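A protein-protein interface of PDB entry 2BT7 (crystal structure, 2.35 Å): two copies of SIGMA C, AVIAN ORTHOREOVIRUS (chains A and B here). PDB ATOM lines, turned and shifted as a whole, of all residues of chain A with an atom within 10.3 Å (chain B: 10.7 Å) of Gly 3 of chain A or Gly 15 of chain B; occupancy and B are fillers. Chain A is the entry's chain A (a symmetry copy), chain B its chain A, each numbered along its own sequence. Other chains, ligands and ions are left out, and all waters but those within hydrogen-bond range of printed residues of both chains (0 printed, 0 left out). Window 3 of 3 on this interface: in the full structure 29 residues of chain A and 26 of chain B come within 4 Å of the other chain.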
ATOM      1  N   SER A   1      35.665 -14.595  -3.353  1.00  0.00           N
ATOM      2  CA  SER A   1      34.729 -13.450  -3.384  1.00  0.00           C
ATOM      3  C   SER A   1      33.320 -13.817  -2.916  1.00  0.00           C
ATOM      4  O   SER A   1      32.704 -14.757  -3.421  1.00  0.00           O
ATOM      5  CB  SER A   1      34.659 -12.813  -4.785  1.00  0.00           C
ATOM      6  OG  SER A   1      33.994 -11.545  -4.753  1.00  0.00           O
ATOM      7  N   HIS A   2      32.844 -13.047  -1.933  1.00  0.00           N
ATOM      8  CA  HIS A   2      31.447 -12.978  -1.520  1.00  0.00           C
ATOM      9  C   HIS A   2      30.755 -12.181  -2.620  1.00  0.00           C
ATOM     10  O   HIS A   2      31.411 -11.518  -3.418  1.00  0.00           O
ATOM     11  CB  HIS A   2      31.379 -12.269  -0.161  1.00  0.00           C
ATOM     12  CG  HIS A   2      32.371 -12.796   0.837  1.00  0.00           C
ATOM     13  ND1 HIS A   2      32.006 -13.566   1.924  1.00  0.00           N
ATOM     14  CD2 HIS A   2      33.723 -12.698   0.890  1.00  0.00           C
ATOM     15  CE1 HIS A   2      33.085 -13.910   2.608  1.00  0.00           C
ATOM     16  NE2 HIS A   2      34.139 -13.387   2.007  1.00  0.00           N
ATOM     17  N   GLY A   3      29.452 -12.253  -2.748  1.00  0.00           N
ATOM     18  CA  GLY A   3      28.883 -11.523  -3.888  1.00  0.00           C
ATOM     19  C   GLY A   3      28.291 -10.209  -3.433  1.00  0.00           C
ATOM     20  O   GLY A   3      28.820  -9.555  -2.530  1.00  0.00           O
ATOM     21  N   LEU A   4      27.179  -9.818  -4.030  1.00  0.00           N
ATOM     22  CA  LEU A   4      26.476  -8.705  -3.443  1.00  0.00           C
ATOM     23  C   LEU A   4      25.147  -9.027  -2.764  1.00  0.00           C
ATOM     24  O   LEU A   4      24.339  -9.870  -3.206  1.00  0.00           O
ATOM     25  CB  LEU A   4      26.533  -7.416  -4.280  1.00  0.00           C
ATOM     26  CG  LEU A   4      25.984  -7.226  -5.681  1.00  0.00           C
ATOM     27  CD1 LEU A   4      26.756  -6.108  -6.315  1.00  0.00           C
ATOM     28  CD2 LEU A   4      26.079  -8.478  -6.529  1.00  0.00           C
ATOM     29  N   SER A   5      25.026  -8.384  -1.606  1.00  0.00           N
ATOM     30  CA  SER A   5      23.945  -8.531  -0.660  1.00  0.00           C
ATOM     31  C   SER A   5      23.214  -7.166  -0.579  1.00  0.00           C
ATOM     32  O   SER A   5      23.820  -6.110  -0.765  1.00  0.00           O
ATOM     33  CB  SER A   5      24.570  -8.896   0.686  1.00  0.00           C
ATOM     34  OG  SER A   5      23.599  -9.342   1.595  1.00  0.00           O
ATOM     35  N   PHE A   6      21.912  -7.195  -0.325  1.00  0.00           N
ATOM     36  CA  PHE A   6      21.122  -5.964  -0.308  1.00  0.00           C
ATOM     37  C   PHE A   6      20.463  -5.688   1.043  1.00  0.00           C
ATOM     38  O   PHE A   6      19.695  -6.514   1.561  1.00  0.00           O
ATOM     39  CB  PHE A   6      20.132  -5.940  -1.478  1.00  0.00           C
ATOM     40  CG  PHE A   6      20.812  -5.891  -2.800  1.00  0.00           C
ATOM     41  CD1 PHE A   6      21.252  -7.073  -3.416  1.00  0.00           C
ATOM     42  CD2 PHE A   6      21.086  -4.668  -3.406  1.00  0.00           C
ATOM     43  CE1 PHE A   6      21.918  -7.038  -4.625  1.00  0.00           C
ATOM     44  CE2 PHE A   6      21.754  -4.617  -4.636  1.00  0.00           C
ATOM     45  CZ  PHE A   6      22.172  -5.803  -5.247  1.00  0.00           C
ATOM     46  N   SER A   7      20.798  -4.526   1.604  1.00  0.00           N
ATOM     47  CA  SER A   7      20.313  -4.108   2.911  1.00  0.00           C
ATOM     48  C   SER A   7      18.998  -3.329   2.798  1.00  0.00           C
ATOM     49  O   SER A   7      18.861  -2.502   1.891  1.00  0.00           O
ATOM     50  CB  SER A   7      21.354  -3.219   3.547  1.00  0.00           C
ATOM     51  OG  SER A   7      21.345  -3.433   4.929  1.00  0.00           O
ATOM     52  N   LEU A  10      16.569  -1.670   0.403  1.00  0.00           N
ATOM     53  CA  LEU A  10      16.858  -2.450  -0.828  1.00  0.00           C
ATOM     54  C   LEU A  10      16.581  -3.926  -0.564  1.00  0.00           C
ATOM     55  O   LEU A  10      16.877  -4.426   0.512  1.00  0.00           O
ATOM     56  CB  LEU A  10      18.303  -2.244  -1.320  1.00  0.00           C
ATOM     57  CG  LEU A  10      18.759  -0.797  -1.531  1.00  0.00           C
ATOM     58  CD1 LEU A  10      20.244  -0.757  -1.782  1.00  0.00           C
ATOM     59  CD2 LEU A  10      17.973  -0.074  -2.660  1.00  0.00           C
ATOM     60  N   VAL A  12      16.139  -8.062  -2.788  1.00  0.00           N
ATOM     61  CA  VAL A  12      16.291  -8.874  -4.014  1.00  0.00           C
ATOM     62  C   VAL A  12      15.415 -10.153  -3.976  1.00  0.00           C
ATOM     63  O   VAL A  12      15.380 -10.874  -2.981  1.00  0.00           O
ATOM     64  CB  VAL A  12      17.805  -9.203  -4.330  1.00  0.00           C
ATOM     65  CG1 VAL A  12      18.485  -9.955  -3.186  1.00  0.00           C
ATOM     66  CG2 VAL A  12      17.945  -9.981  -5.656  1.00  0.00           C
ATOM     67  N   LEU B   4      29.227  -4.151 -11.668  1.00  0.00           N
ATOM     68  CA  LEU B   4      28.350  -3.090 -11.238  1.00  0.00           C
ATOM     69  C   LEU B   4      28.880  -2.185 -10.128  1.00  0.00           C
ATOM     70  O   LEU B   4      29.563  -2.602  -9.171  1.00  0.00           O
ATOM     71  CB  LEU B   4      26.870  -3.496 -11.154  1.00  0.00           C
ATOM     72  CG  LEU B   4      26.278  -4.564 -10.255  1.00  0.00           C
ATOM     73  CD1 LEU B   4      25.010  -5.039 -10.899  1.00  0.00           C
ATOM     74  CD2 LEU B   4      27.217  -5.730 -10.020  1.00  0.00           C
ATOM     75  N   PHE B   6      27.908   1.499  -7.835  1.00  0.00           N
ATOM     76  CA  PHE B   6      26.749   2.097  -7.172  1.00  0.00           C
ATOM     77  C   PHE B   6      26.900   3.599  -6.933  1.00  0.00           C
ATOM     78  O   PHE B   6      27.854   4.051  -6.281  1.00  0.00           O
ATOM     79  CB  PHE B   6      26.390   1.318  -5.902  1.00  0.00           C
ATOM     80  CG  PHE B   6      25.939  -0.070  -6.190  1.00  0.00           C
ATOM     81  CD1 PHE B   6      26.876  -1.100  -6.357  1.00  0.00           C
ATOM     82  CD2 PHE B   6      24.587  -0.345  -6.375  1.00  0.00           C
ATOM     83  CE1 PHE B   6      26.472  -2.385  -6.664  1.00  0.00           C
ATOM     84  CE2 PHE B   6      24.161  -1.644  -6.679  1.00  0.00           C
ATOM     85  CZ  PHE B   6      25.104  -2.667  -6.824  1.00  0.00           C
ATOM     86  N   SER B  11      25.166   2.837  -2.012  1.00  0.00           N
ATOM     87  CA  SER B  11      26.580   2.567  -1.739  1.00  0.00           C
ATOM     88  C   SER B  11      26.825   1.081  -1.416  1.00  0.00           C
ATOM     89  O   SER B  11      25.895   0.359  -1.055  1.00  0.00           O
ATOM     90  CB  SER B  11      27.114   3.491  -0.625  1.00  0.00           C
ATOM     91  OG  SER B  11      26.623   3.123   0.660  1.00  0.00           O
ATOM     92  N   VAL B  12      28.080   0.645  -1.559  1.00  0.00           N
ATOM     93  CA  VAL B  12      28.486  -0.754  -1.307  1.00  0.00           C
ATOM     94  C   VAL B  12      29.730  -0.841  -0.385  1.00  0.00           C
ATOM     95  O   VAL B  12      30.715  -0.132  -0.575  1.00  0.00           O
ATOM     96  CB  VAL B  12      28.684  -1.571  -2.647  1.00  0.00           C
ATOM     97  CG1 VAL B  12      29.734  -0.938  -3.560  1.00  0.00           C
ATOM     98  CG2 VAL B  12      29.027  -3.048  -2.358  1.00  0.00           C
ATOM     99  N   ALA B  13      29.660  -1.684   0.637  1.00  0.00           N
ATOM    100  CA  ALA B  13      30.790  -1.860   1.533  1.00  0.00           C
ATOM    101  C   ALA B  13      30.796  -3.305   1.954  1.00  0.00           C
ATOM    102  O   ALA B  13      29.800  -3.784   2.478  1.00  0.00           O
ATOM    103  CB  ALA B  13      30.690  -0.939   2.754  1.00  0.00           C
ATOM    104  N   ASP B  14      31.923  -3.989   1.705  1.00  0.00           N
ATOM    105  CA  ASP B  14      32.094  -5.429   1.990  1.00  0.00           C
ATOM    106  C   ASP B  14      31.002  -6.298   1.350  1.00  0.00           C
ATOM    107  O   ASP B  14      30.431  -7.164   2.003  1.00  0.00           O
ATOM    108  CB  ASP B  14      32.122  -5.688   3.502  1.00  0.00           C
ATOM    109  CG  ASP B  14      33.168  -4.855   4.227  1.00  0.00           C
ATOM    110  OD1 ASP B  14      33.003  -3.613   4.329  1.00  0.00           O
ATOM    111  OD2 ASP B  14      34.152  -5.456   4.716  1.00  0.00           O
ATOM    112  N   GLY B  15      30.694  -6.059   0.084  1.00  0.00           N
ATOM    113  CA  GLY B  15      29.636  -6.818  -0.574  1.00  0.00           C
ATOM    114  C   GLY B  15      28.199  -6.417  -0.244  1.00  0.00           C
ATOM    115  O   GLY B  15      27.273  -6.843  -0.941  1.00  0.00           O
ATOM    116  N   VAL B  16      27.993  -5.620   0.809  1.00  0.00           N
ATOM    117  CA  VAL B  16      26.635  -5.161   1.181  1.00  0.00           C
ATOM    118  C   VAL B  16      26.268  -3.833   0.510  1.00  0.00           C
ATOM    119  O   VAL B  16      26.980  -2.836   0.627  1.00  0.00           O
ATOM    120  CB  VAL B  16      26.438  -5.070   2.695  1.00  0.00           C
ATOM    121  CG1 VAL B  16      24.950  -4.812   3.022  1.00  0.00           C
ATOM    122  CG2 VAL B  16      26.934  -6.365   3.368  1.00  0.00           C
ATOM    123  N   VAL B  17      25.174  -3.850  -0.231  1.00  0.00           N
ATOM    124  CA  VAL B  17      24.679  -2.663  -0.919  1.00  0.00           C
ATOM    125  C   VAL B  17      23.608  -2.000  -0.020  1.00  0.00           C
ATOM    126  O   VAL B  17      22.704  -2.679   0.479  1.00  0.00           O
ATOM    127  CB  VAL B  17      24.119  -3.017  -2.326  1.00  0.00           C
ATOM    128  CG1 VAL B  17      23.583  -1.777  -3.058  1.00  0.00           C
ATOM    129  CG2 VAL B  17      25.191  -3.696  -3.175  1.00  0.00           C
ATOM    130  N   SER B  18      23.739  -0.686   0.185  1.00  0.00           N
ATOM    131  CA  SER B  18      22.842   0.100   1.058  1.00  0.00           C
ATOM    132  C   SER B  18      22.263   1.351   0.402  1.00  0.00           C
ATOM    133  O   SER B  18      22.841   1.929  -0.530  1.00  0.00           O
ATOM    134  CB  SER B  18      23.588   0.564   2.304  1.00  0.00           C
ATOM    135  OG  SER B  18      23.923  -0.517   3.145  1.00  0.00           O
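The backbone carbonyl oxygen of Ser 5 of chain A lies within hydrogen-bond range of the backbone NH of Val 17 of chain B, at 2.7 Å. N of Ser 5 of chain A sits at hydrogen-bond distance from O of Gly 15 of chain B, 2.8 Å away. N of Ser 7 of chain A sits at hydrogen-bond distance from O of Val 17 of chain B, at 2.9 Å.
The backbone carbonyl oxygen (O) of Ser 11 of chain B lies within hydrogen-bond range of the backbone NH (N) of Ser 18 of chain B (2.7 Å).
Among the printed residues, merely in contact across the chains: Gly 3 of chain A with Gly 15 of chain B (3.5 Å), Leu 4 of chain A with Leu 4 of chain B (3.8 Å), Leu 4 of chain A with Phe 6 of chain B (3.8 Å), Leu 4 of chain A with Gly 15 of chain B (3.2 Å), Ser 5 of chain A with Val 16 of chain B (3.6 Å), Phe 6 of chain A with Val 17 of chain B (3.6 Å), Ser 7 of chain A with Val 16 of chain B (3.97 Å), Ser 7 of chain A with Ser 18 of chain B (3.7 Å), Leu 10 of chain A with Val 17 of chain B (3.7 Å) and Leu 10 of chain A with Ser 18 of chain B (3.6 Å).
Of chain B, only Leu 4, Phe 6 and Gly 15 come within 4 Å of Leu 4 of chain A. Of chain B, only Gly 15, Val 16 and Val 17 come within 4 Å of Ser 5 of chain A. Of the printed residues of chain B, Phe 6 of chain A touches Val 17 (3.6 Å). Printed residues of chain B within 4 Å of Ser 7 of chain A: Val 16, Val 17 and Ser 18. Of the printed residues of chain B, Leu 10 of chain A touches Val 17 (3.7 Å) and Ser 18 (3.6 Å). Of the printed residues of chain A, Phe 6 of chain B touches Leu 4. Ser 11 of chain B touches none of the printed residues of chain A. No residue of chain A comes within 4 Å of Ala 13 of chain B. Printed residues of chain A within 4 Å of Ser 18 of chain B: Ser 7 and Leu 10. The nearest residue of chain A that does not touch Gly 15 of chain B is Phe 6 of chain A (5.4 Å). The nearest printed residue of chain B that does not touch Phe 6 of chain A is Phe 6 of chain B (4.3 Å).
Of the 10 printed residues of chain B, 6 touch a printed residue of chain A. Hydrophobic or aromatic side chains of chain B that line the printed part of chain A: Leu 4, Phe 6, Val 16 and Val 17. Along chain A the printed residues that touch a printed residue of chain B span positions 3 to 10. Among the printed residues, no Asp or Glu carboxylate lies within 4 Å of a Lys or Arg side-chain nitrogen of the other chain.
Leu 4 of chain A touches its own counterpart, Leu 4 of chain B. Leu 4 of chain A touches Phe 6 of chain B, but with the chains exchanged Phe 6 of chain A does not touch Leu 4 of chain B (6.4 Å). Of the 13 pairs that touch across the chains among the printed residues, 1 has its exchanged pair printed and touching as well.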
